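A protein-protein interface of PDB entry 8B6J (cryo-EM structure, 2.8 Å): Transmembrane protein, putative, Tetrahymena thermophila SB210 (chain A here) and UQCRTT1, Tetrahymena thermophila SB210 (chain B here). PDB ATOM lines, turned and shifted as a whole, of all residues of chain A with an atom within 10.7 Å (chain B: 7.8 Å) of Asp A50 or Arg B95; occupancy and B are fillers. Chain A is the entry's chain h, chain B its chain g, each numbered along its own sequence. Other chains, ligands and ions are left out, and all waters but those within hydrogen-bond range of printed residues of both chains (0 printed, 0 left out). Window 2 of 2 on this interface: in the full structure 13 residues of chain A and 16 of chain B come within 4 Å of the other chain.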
ATOM      1  N   TYR A  38      11.964   5.783   4.549  1.00  0.00           N
ATOM      2  CA  TYR A  38      11.294   7.009   4.958  1.00  0.00           C
ATOM      3  C   TYR A  38       9.796   6.927   4.705  1.00  0.00           C
ATOM      4  O   TYR A  38       9.330   6.236   3.797  1.00  0.00           O
ATOM      5  CB  TYR A  38      11.865   8.207   4.204  1.00  0.00           C
ATOM      6  CG  TYR A  38      13.363   8.350   4.310  1.00  0.00           C
ATOM      7  CD1 TYR A  38      14.053   7.872   5.413  1.00  0.00           C
ATOM      8  CD2 TYR A  38      14.087   8.965   3.302  1.00  0.00           C
ATOM      9  CE1 TYR A  38      15.419   8.003   5.509  1.00  0.00           C
ATOM     10  CE2 TYR A  38      15.450   9.103   3.391  1.00  0.00           C
ATOM     11  CZ  TYR A  38      16.113   8.618   4.494  1.00  0.00           C
ATOM     12  OH  TYR A  38      17.478   8.753   4.579  1.00  0.00           O
ATOM     13  N   GLY A  39       9.037   7.652   5.524  1.00  0.00           N
ATOM     14  CA  GLY A  39       7.619   7.812   5.283  1.00  0.00           C
ATOM     15  C   GLY A  39       6.769   6.606   5.599  1.00  0.00           C
ATOM     16  O   GLY A  39       5.657   6.498   5.082  1.00  0.00           O
ATOM     17  N   SER A  40       7.256   5.694   6.435  1.00  0.00           N
ATOM     18  CA  SER A  40       6.505   4.513   6.834  1.00  0.00           C
ATOM     19  C   SER A  40       6.304   4.537   8.341  1.00  0.00           C
ATOM     20  O   SER A  40       7.262   4.726   9.096  1.00  0.00           O
ATOM     21  CB  SER A  40       7.227   3.229   6.415  1.00  0.00           C
ATOM     22  OG  SER A  40       8.499   3.135   7.028  1.00  0.00           O
ATOM     23  N   VAL A  41       5.056   4.351   8.770  1.00  0.00           N
ATOM     24  CA  VAL A  41       4.759   4.318  10.199  1.00  0.00           C
ATOM     25  C   VAL A  41       5.463   3.141  10.859  1.00  0.00           C
ATOM     26  O   VAL A  41       5.917   3.233  12.006  1.00  0.00           O
ATOM     27  CB  VAL A  41       3.237   4.266  10.420  1.00  0.00           C
ATOM     28  CG1 VAL A  41       2.918   3.923  11.859  1.00  0.00           C
ATOM     29  CG2 VAL A  41       2.607   5.593  10.039  1.00  0.00           C
ATOM     30  N   SER A  44       8.968   3.950  12.320  1.00  0.00           N
ATOM     31  CA  SER A  44       9.071   4.649  13.591  1.00  0.00           C
ATOM     32  C   SER A  44       7.717   5.228  13.970  1.00  0.00           C
ATOM     33  O   SER A  44       6.901   5.553  13.104  1.00  0.00           O
ATOM     34  CB  SER A  44      10.114   5.768  13.530  1.00  0.00           C
ATOM     35  OG  SER A  44       9.860   6.740  14.525  1.00  0.00           O
ATOM     36  N   VAL A  45       7.496   5.357  15.282  1.00  0.00           N
ATOM     37  CA  VAL A  45       6.290   6.004  15.796  1.00  0.00           C
ATOM     38  C   VAL A  45       6.378   7.520  15.750  1.00  0.00           C
ATOM     39  O   VAL A  45       5.397   8.197  16.082  1.00  0.00           O
ATOM     40  CB  VAL A  45       5.995   5.570  17.246  1.00  0.00           C
ATOM     41  CG1 VAL A  45       5.585   4.110  17.287  1.00  0.00           C
ATOM     42  CG2 VAL A  45       7.202   5.809  18.141  1.00  0.00           C
ATOM     43  N   ARG A  46       7.524   8.077  15.360  1.00  0.00           N
ATOM     44  CA  ARG A  46       7.665   9.521  15.247  1.00  0.00           C
ATOM     45  C   ARG A  46       6.972  10.091  14.018  1.00  0.00           C
ATOM     46  O   ARG A  46       6.861  11.315  13.905  1.00  0.00           O
ATOM     47  CB  ARG A  46       9.146   9.904  15.213  1.00  0.00           C
ATOM     48  CG  ARG A  46       9.889   9.625  16.503  1.00  0.00           C
ATOM     49  CD  ARG A  46      11.280  10.231  16.474  1.00  0.00           C
ATOM     50  NE  ARG A  46      12.007   9.988  17.714  1.00  0.00           N
ATOM     51  CZ  ARG A  46      11.921  10.750  18.795  1.00  0.00           C
ATOM     52  NH1 ARG A  46      11.146  11.821  18.827  1.00  0.00           N
ATOM     53  NH2 ARG A  46      12.629  10.427  19.873  1.00  0.00           N
ATOM     54  N   TYR A  47       6.510   9.244  13.100  1.00  0.00           N
ATOM     55  CA  TYR A  47       5.860   9.724  11.889  1.00  0.00           C
ATOM     56  C   TYR A  47       4.412  10.137  12.109  1.00  0.00           C
ATOM     57  O   TYR A  47       3.809  10.715  11.199  1.00  0.00           O
ATOM     58  CB  TYR A  47       5.927   8.652  10.800  1.00  0.00           C
ATOM     59  CG  TYR A  47       7.277   8.561  10.130  1.00  0.00           C
ATOM     60  CD1 TYR A  47       7.652   9.479   9.162  1.00  0.00           C
ATOM     61  CD2 TYR A  47       8.174   7.559  10.464  1.00  0.00           C
ATOM     62  CE1 TYR A  47       8.884   9.403   8.547  1.00  0.00           C
ATOM     63  CE2 TYR A  47       9.409   7.474   9.854  1.00  0.00           C
ATOM     64  CZ  TYR A  47       9.757   8.399   8.896  1.00  0.00           C
ATOM     65  OH  TYR A  47      10.986   8.320   8.284  1.00  0.00           O
ATOM     66  N   TYR A  48       3.837   9.860  13.280  1.00  0.00           N
ATOM     67  CA  TYR A  48       2.486  10.335  13.558  1.00  0.00           C
ATOM     68  C   TYR A  48       2.451  11.849  13.718  1.00  0.00           C
ATOM     69  O   TYR A  48       1.424  12.477  13.437  1.00  0.00           O
ATOM     70  CB  TYR A  48       1.936   9.656  14.809  1.00  0.00           C
ATOM     71  CG  TYR A  48       1.737   8.168  14.649  1.00  0.00           C
ATOM     72  CD1 TYR A  48       0.670   7.667  13.919  1.00  0.00           C
ATOM     73  CD2 TYR A  48       2.616   7.266  15.226  1.00  0.00           C
ATOM     74  CE1 TYR A  48       0.486   6.311  13.768  1.00  0.00           C
ATOM     75  CE2 TYR A  48       2.440   5.909  15.082  1.00  0.00           C
ATOM     76  CZ  TYR A  48       1.375   5.438  14.352  1.00  0.00           C
ATOM     77  OH  TYR A  48       1.194   4.081  14.210  1.00  0.00           O
ATOM     78  N   HIS A  49       3.552  12.448  14.171  1.00  0.00           N
ATOM     79  CA  HIS A  49       3.665  13.901  14.287  1.00  0.00           C
ATOM     80  C   HIS A  49       4.233  14.428  12.973  1.00  0.00           C
ATOM     81  O   HIS A  49       5.434  14.660  12.821  1.00  0.00           O
ATOM     82  CB  HIS A  49       4.538  14.273  15.478  1.00  0.00           C
ATOM     83  CG  HIS A  49       4.649  15.746  15.711  1.00  0.00           C
ATOM     84  ND1 HIS A  49       3.556  16.541  15.980  1.00  0.00           N
ATOM     85  CD2 HIS A  49       5.724  16.569  15.719  1.00  0.00           C
ATOM     86  CE1 HIS A  49       3.952  17.791  16.141  1.00  0.00           C
ATOM     87  NE2 HIS A  49       5.263  17.835  15.988  1.00  0.00           N
ATOM     88  N   ASP A  50       3.342  14.612  12.002  1.00  0.00           N
ATOM     89  CA  ASP A  50       3.742  14.893  10.626  1.00  0.00           C
ATOM     90  C   ASP A  50       2.914  16.031  10.034  1.00  0.00           C
ATOM     91  O   ASP A  50       2.423  15.951   8.908  1.00  0.00           O
ATOM     92  CB  ASP A  50       3.611  13.635   9.772  1.00  0.00           C
ATOM     93  CG  ASP A  50       2.197  13.094   9.752  1.00  0.00           C
ATOM     94  OD1 ASP A  50       1.330  13.660  10.450  1.00  0.00           O
ATOM     95  OD2 ASP A  50       1.950  12.102   9.037  1.00  0.00           O
ATOM     96  N   LYS A  51       2.749  17.111  10.790  1.00  0.00           N
ATOM     97  CA  LYS A  51       2.086  18.290  10.255  1.00  0.00           C
ATOM     98  C   LYS A  51       3.035  19.064   9.348  1.00  0.00           C
ATOM     99  O   LYS A  51       4.256  19.041   9.527  1.00  0.00           O
ATOM    100  CB  LYS A  51       1.584  19.190  11.383  1.00  0.00           C
ATOM    101  CG  LYS A  51       0.403  18.616  12.141  1.00  0.00           C
ATOM    102  CD  LYS A  51      -0.233  19.652  13.049  1.00  0.00           C
ATOM    103  CE  LYS A  51      -1.496  19.113  13.696  1.00  0.00           C
ATOM    104  NZ  LYS A  51      -2.159  20.129  14.556  1.00  0.00           N
ATOM    105  N   MET A  52       2.461  19.751   8.363  1.00  0.00           N
ATOM    106  CA  MET A  52       3.273  20.492   7.405  1.00  0.00           C
ATOM    107  C   MET A  52       4.085  21.566   8.117  1.00  0.00           C
ATOM    108  O   MET A  52       3.546  22.360   8.892  1.00  0.00           O
ATOM    109  CB  MET A  52       2.383  21.127   6.336  1.00  0.00           C
ATOM    110  CG  MET A  52       3.129  22.043   5.373  1.00  0.00           C
ATOM    111  SD  MET A  52       2.132  22.583   3.970  1.00  0.00           S
ATOM    112  CE  MET A  52       0.850  23.523   4.792  1.00  0.00           C
ATOM    113  N   SER A  53       5.388  21.588   7.845  1.00  0.00           N
ATOM    114  CA  SER A  53       6.270  22.597   8.428  1.00  0.00           C
ATOM    115  C   SER A  53       7.531  22.661   7.578  1.00  0.00           C
ATOM    116  O   SER A  53       8.283  21.684   7.515  1.00  0.00           O
ATOM    117  CB  SER A  53       6.598  22.260   9.875  1.00  0.00           C
ATOM    118  OG  SER A  53       7.299  21.033   9.966  1.00  0.00           O
ATOM    119  N   TYR A  54       7.758  23.803   6.935  1.00  0.00           N
ATOM    120  CA  TYR A  54       8.941  24.018   6.116  1.00  0.00           C
ATOM    121  C   TYR A  54       9.511  25.391   6.432  1.00  0.00           C
ATOM    122  O   TYR A  54       8.763  26.357   6.597  1.00  0.00           O
ATOM    123  CB  TYR A  54       8.612  23.910   4.623  1.00  0.00           C
ATOM    124  CG  TYR A  54       9.819  23.986   3.720  1.00  0.00           C
ATOM    125  CD1 TYR A  54      10.591  22.863   3.469  1.00  0.00           C
ATOM    126  CD2 TYR A  54      10.183  25.178   3.112  1.00  0.00           C
ATOM    127  CE1 TYR A  54      11.693  22.924   2.643  1.00  0.00           C
ATOM    128  CE2 TYR A  54      11.282  25.248   2.284  1.00  0.00           C
ATOM    129  CZ  TYR A  54      12.034  24.119   2.054  1.00  0.00           C
ATOM    130  OH  TYR A  54      13.132  24.181   1.230  1.00  0.00           O
ATOM    131  N   MET B  89      -8.470  29.482   5.719  1.00  0.00           N
ATOM    132  CA  MET B  89      -9.062  29.223   7.022  1.00  0.00           C
ATOM    133  C   MET B  89      -8.074  28.480   7.909  1.00  0.00           C
ATOM    134  O   MET B  89      -7.257  27.683   7.440  1.00  0.00           O
ATOM    135  CB  MET B  89     -10.347  28.412   6.875  1.00  0.00           C
ATOM    136  CG  MET B  89     -11.466  29.160   6.179  1.00  0.00           C
ATOM    137  SD  MET B  89     -12.986  28.200   6.070  1.00  0.00           S
ATOM    138  CE  MET B  89     -13.433  28.070   7.797  1.00  0.00           C
ATOM    139  N   ASP B  90      -8.145  28.759   9.212  1.00  0.00           N
ATOM    140  CA  ASP B  90      -7.268  28.077  10.157  1.00  0.00           C
ATOM    141  C   ASP B  90      -7.399  26.565  10.040  1.00  0.00           C
ATOM    142  O   ASP B  90      -6.425  25.839  10.269  1.00  0.00           O
ATOM    143  CB  ASP B  90      -7.575  28.533  11.584  1.00  0.00           C
ATOM    144  CG  ASP B  90      -9.062  28.633  11.859  1.00  0.00           C
ATOM    145  OD1 ASP B  90      -9.740  27.583  11.862  1.00  0.00           O
ATOM    146  OD2 ASP B  90      -9.551  29.762  12.069  1.00  0.00           O
ATOM    147  N   ARG B  91      -8.583  26.075   9.672  1.00  0.00           N
ATOM    148  CA  ARG B  91      -8.750  24.647   9.426  1.00  0.00           C
ATOM    149  C   ARG B  91      -7.809  24.176   8.324  1.00  0.00           C
ATOM    150  O   ARG B  91      -7.085  23.187   8.488  1.00  0.00           O
ATOM    151  CB  ARG B  91     -10.206  24.355   9.063  1.00  0.00           C
ATOM    152  CG  ARG B  91     -10.580  22.880   9.060  1.00  0.00           C
ATOM    153  CD  ARG B  91     -10.310  22.206   7.720  1.00  0.00           C
ATOM    154  NE  ARG B  91     -11.047  22.827   6.628  1.00  0.00           N
ATOM    155  CZ  ARG B  91     -11.016  22.407   5.371  1.00  0.00           C
ATOM    156  NH1 ARG B  91     -10.294  21.358   5.009  1.00  0.00           N
ATOM    157  NH2 ARG B  91     -11.725  23.056   4.451  1.00  0.00           N
ATOM    158  N   GLU B  92      -7.805  24.878   7.189  1.00  0.00           N
ATOM    159  CA  GLU B  92      -6.909  24.513   6.098  1.00  0.00           C
ATOM    160  C   GLU B  92      -5.452  24.693   6.500  1.00  0.00           C
ATOM    161  O   GLU B  92      -4.599  23.861   6.169  1.00  0.00           O
ATOM    162  CB  GLU B  92      -7.223  25.351   4.860  1.00  0.00           C
ATOM    163  CG  GLU B  92      -8.665  25.264   4.401  1.00  0.00           C
ATOM    164  CD  GLU B  92      -8.944  26.158   3.213  1.00  0.00           C
ATOM    165  OE1 GLU B  92      -7.987  26.757   2.682  1.00  0.00           O
ATOM    166  OE2 GLU B  92     -10.121  26.264   2.811  1.00  0.00           O
ATOM    167  N   LEU B  93      -5.149  25.778   7.213  1.00  0.00           N
ATOM    168  CA  LEU B  93      -3.767  26.059   7.588  1.00  0.00           C
ATOM    169  C   LEU B  93      -3.207  24.967   8.491  1.00  0.00           C
ATOM    170  O   LEU B  93      -2.037  24.588   8.366  1.00  0.00           O
ATOM    171  CB  LEU B  93      -3.684  27.418   8.281  1.00  0.00           C
ATOM    172  CG  LEU B  93      -2.629  28.397   7.766  1.00  0.00           C
ATOM    173  CD1 LEU B  93      -2.903  28.786   6.324  1.00  0.00           C
ATOM    174  CD2 LEU B  93      -2.582  29.631   8.651  1.00  0.00           C
ATOM    175  N   ARG B  94      -4.026  24.448   9.407  1.00  0.00           N
ATOM    176  CA  ARG B  94      -3.543  23.471  10.376  1.00  0.00           C
ATOM    177  C   ARG B  94      -3.496  22.067   9.783  1.00  0.00           C
ATOM    178  O   ARG B  94      -2.427  21.453   9.702  1.00  0.00           O
ATOM    179  CB  ARG B  94      -4.433  23.491  11.620  1.00  0.00           C
ATOM    180  CG  ARG B  94      -3.840  22.770  12.817  1.00  0.00           C
ATOM    181  CD  ARG B  94      -4.888  22.492  13.883  1.00  0.00           C
ATOM    182  NE  ARG B  94      -5.728  23.653  14.155  1.00  0.00           N
ATOM    183  CZ  ARG B  94      -6.913  23.877  13.604  1.00  0.00           C
ATOM    184  NH1 ARG B  94      -7.447  23.032  12.735  1.00  0.00           N
ATOM    185  NH2 ARG B  94      -7.584  24.976  13.934  1.00  0.00           N
ATOM    186  N   ARG B  95      -4.648  21.543   9.362  1.00  0.00           N
ATOM    187  CA  ARG B  95      -4.763  20.147   8.933  1.00  0.00           C
ATOM    188  C   ARG B  95      -5.756  20.067   7.779  1.00  0.00           C
ATOM    189  O   ARG B  95      -6.972  20.076   7.994  1.00  0.00           O
ATOM    190  CB  ARG B  95      -5.198  19.260  10.094  1.00  0.00           C
ATOM    191  CG  ARG B  95      -4.091  18.395  10.666  1.00  0.00           C
ATOM    192  CD  ARG B  95      -3.946  17.104   9.888  1.00  0.00           C
ATOM    193  NE  ARG B  95      -2.895  16.252  10.433  1.00  0.00           N
ATOM    194  CZ  ARG B  95      -1.655  16.185   9.967  1.00  0.00           C
ATOM    195  NH1 ARG B  95      -1.261  16.913   8.935  1.00  0.00           N
ATOM    196  NH2 ARG B  95      -0.789  15.362  10.548  1.00  0.00           N
ATOM    197  N   CYS B  96      -5.233  19.987   6.558  1.00  0.00           N
ATOM    198  CA  CYS B  96      -6.059  19.744   5.379  1.00  0.00           C
ATOM    199  C   CYS B  96      -5.143  19.246   4.276  1.00  0.00           C
ATOM    200  O   CYS B  96      -4.244  19.975   3.845  1.00  0.00           O
ATOM    201  CB  CYS B  96      -6.794  21.010   4.946  1.00  0.00           C
ATOM    202  SG  CYS B  96      -7.880  20.779   3.521  1.00  0.00           S
ATOM    203  N   TYR B  97      -5.357  18.009   3.825  1.00  0.00           N
ATOM    204  CA  TYR B  97      -4.422  17.416   2.877  1.00  0.00           C
ATOM    205  C   TYR B  97      -4.594  18.001   1.481  1.00  0.00           C
ATOM    206  O   TYR B  97      -3.615  18.152   0.744  1.00  0.00           O
ATOM    207  CB  TYR B  97      -4.589  15.898   2.845  1.00  0.00           C
ATOM    208  CG  TYR B  97      -3.406  15.194   2.229  1.00  0.00           C
ATOM    209  CD1 TYR B  97      -2.239  15.001   2.952  1.00  0.00           C
ATOM    210  CD2 TYR B  97      -3.450  14.730   0.924  1.00  0.00           C
ATOM    211  CE1 TYR B  97      -1.152  14.362   2.395  1.00  0.00           C
ATOM    212  CE2 TYR B  97      -2.368  14.091   0.359  1.00  0.00           C
ATOM    213  CZ  TYR B  97      -1.221  13.909   1.099  1.00  0.00           C
ATOM    214  OH  TYR B  97      -0.139  13.270   0.542  1.00  0.00           O
ATOM    215  N   PHE B  98      -5.827  18.329   1.091  1.00  0.00           N
ATOM    216  CA  PHE B  98      -6.033  18.958  -0.209  1.00  0.00           C
ATOM    217  C   PHE B  98      -5.330  20.306  -0.271  1.00  0.00           C
ATOM    218  O   PHE B  98      -4.610  20.605  -1.233  1.00  0.00           O
ATOM    219  CB  PHE B  98      -7.527  19.115  -0.486  1.00  0.00           C
ATOM    220  CG  PHE B  98      -7.833  19.820  -1.774  1.00  0.00           C
ATOM    221  CD1 PHE B  98      -7.534  19.232  -2.991  1.00  0.00           C
ATOM    222  CD2 PHE B  98      -8.426  21.070  -1.771  1.00  0.00           C
ATOM    223  CE1 PHE B  98      -7.814  19.880  -4.176  1.00  0.00           C
ATOM    224  CE2 PHE B  98      -8.710  21.721  -2.955  1.00  0.00           C
ATOM    225  CZ  PHE B  98      -8.404  21.123  -4.158  1.00  0.00           C
ATOM    226  N   PHE B  99      -5.515  21.131   0.760  1.00  0.00           N
ATOM    227  CA  PHE B  99      -4.833  22.417   0.804  1.00  0.00           C
ATOM    228  C   PHE B  99      -3.325  22.232   0.850  1.00  0.00           C
ATOM    229  O   PHE B  99      -2.585  22.965   0.188  1.00  0.00           O
ATOM    230  CB  PHE B  99      -5.305  23.225   2.011  1.00  0.00           C
ATOM    231  CG  PHE B  99      -4.499  24.468   2.256  1.00  0.00           C
ATOM    232  CD1 PHE B  99      -4.790  25.641   1.584  1.00  0.00           C
ATOM    233  CD2 PHE B  99      -3.446  24.461   3.154  1.00  0.00           C
ATOM    234  CE1 PHE B  99      -4.049  26.782   1.804  1.00  0.00           C
ATOM    235  CE2 PHE B  99      -2.701  25.600   3.377  1.00  0.00           C
ATOM    236  CZ  PHE B  99      -3.003  26.760   2.702  1.00  0.00           C
ATOM    237  N   GLU B 100      -2.850  21.261   1.630  1.00  0.00           N
ATOM    238  CA  GLU B 100      -1.413  21.029   1.722  1.00  0.00           C
ATOM    239  C   GLU B 100      -0.829  20.671   0.362  1.00  0.00           C
ATOM    240  O   GLU B 100       0.199  21.218  -0.049  1.00  0.00           O
ATOM    241  CB  GLU B 100      -1.129  19.922   2.740  1.00  0.00           C
ATOM    242  CG  GLU B 100       0.322  19.479   2.791  1.00  0.00           C
ATOM    243  CD  GLU B 100       0.595  18.502   3.917  1.00  0.00           C
ATOM    244  OE1 GLU B 100      -0.285  18.334   4.785  1.00  0.00           O
ATOM    245  OE2 GLU B 100       1.690  17.902   3.930  1.00  0.00           O
ATOM    246  N   ARG B 104       1.748  22.955  -1.785  1.00  0.00           N
ATOM    247  CA  ARG B 104       3.066  22.435  -2.128  1.00  0.00           C
ATOM    248  C   ARG B 104       3.298  22.480  -3.631  1.00  0.00           C
ATOM    249  O   ARG B 104       4.390  22.837  -4.088  1.00  0.00           O
ATOM    250  CB  ARG B 104       3.224  21.008  -1.607  1.00  0.00           C
ATOM    251  CG  ARG B 104       3.408  20.917  -0.105  1.00  0.00           C
ATOM    252  CD  ARG B 104       3.718  19.499   0.330  1.00  0.00           C
ATOM    253  NE  ARG B 104       3.882  19.394   1.775  1.00  0.00           N
ATOM    254  CZ  ARG B 104       5.015  19.625   2.424  1.00  0.00           C
ATOM    255  NH1 ARG B 104       6.115  19.990   1.787  1.00  0.00           N
ATOM    256  NH2 ARG B 104       5.045  19.486   3.745  1.00  0.00           N
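NH2 of Arg B95 lies within salt-bridge range of OD1 of Asp A50, 2.7 Å away.
The side-chain carboxylate of Asp B90 lies within salt-bridge range of the guanidinium group of Arg B94, 3.97 Å away.
OE2 of Glu B100 is in salt-bridge range of NE of Arg B104 (3.4 Å).
Among the printed residues, merely in contact across the chains: Lys A51 with Arg B94, Lys A51 with Arg B95, Met A52 with Glu B100 and Met A52 with Arg B104.
Asp A50 touches just one residue of chain B: Arg B95 (2.7 Å).
Arg B95 touches just these residues of chain A: Asp A50 (2.7 Å) and Lys A51 (3.8 Å).
Arg B91 touches none of the printed residues of chain A.
Arg B94 touches one residue of chain A.
No residue of chain A comes within 4 Å of Cys B96.
Printed residues of chain B within 4 Å of Lys A51: Arg B94 and Arg B95.
Printed residues of chain A within 4 Å of Arg B104: Met A52 (3.6 Å).
Printed residues of chain B within 4 Å of Met A52: Glu B100 and Arg B104.
Of the printed residues of chain A, Glu B100 touches Met A52.
Phe B98 touches none of the printed residues of chain A.
Tyr A38 touches none of the printed residues of chain B.
The nearest residue of chain A that does not touch Arg B95 is Tyr A48 (4.6 Å).
Of the 13 printed residues of chain B, 4 touch a printed residue of chain A.
Along chain B the printed residues that touch a printed residue of chain A span positions 94 to 104.
Hydrophobic or aromatic side chains of chain A that line the printed part of chain B: Met A52.
Among the printed residues, 5 pairs touch across the chains.
Among the printed residues, Asp or Glu carboxylates within 4 Å of a Lys or Arg side-chain nitrogen of the other chain: Asp A50 with Arg B95 (2.7 Å).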
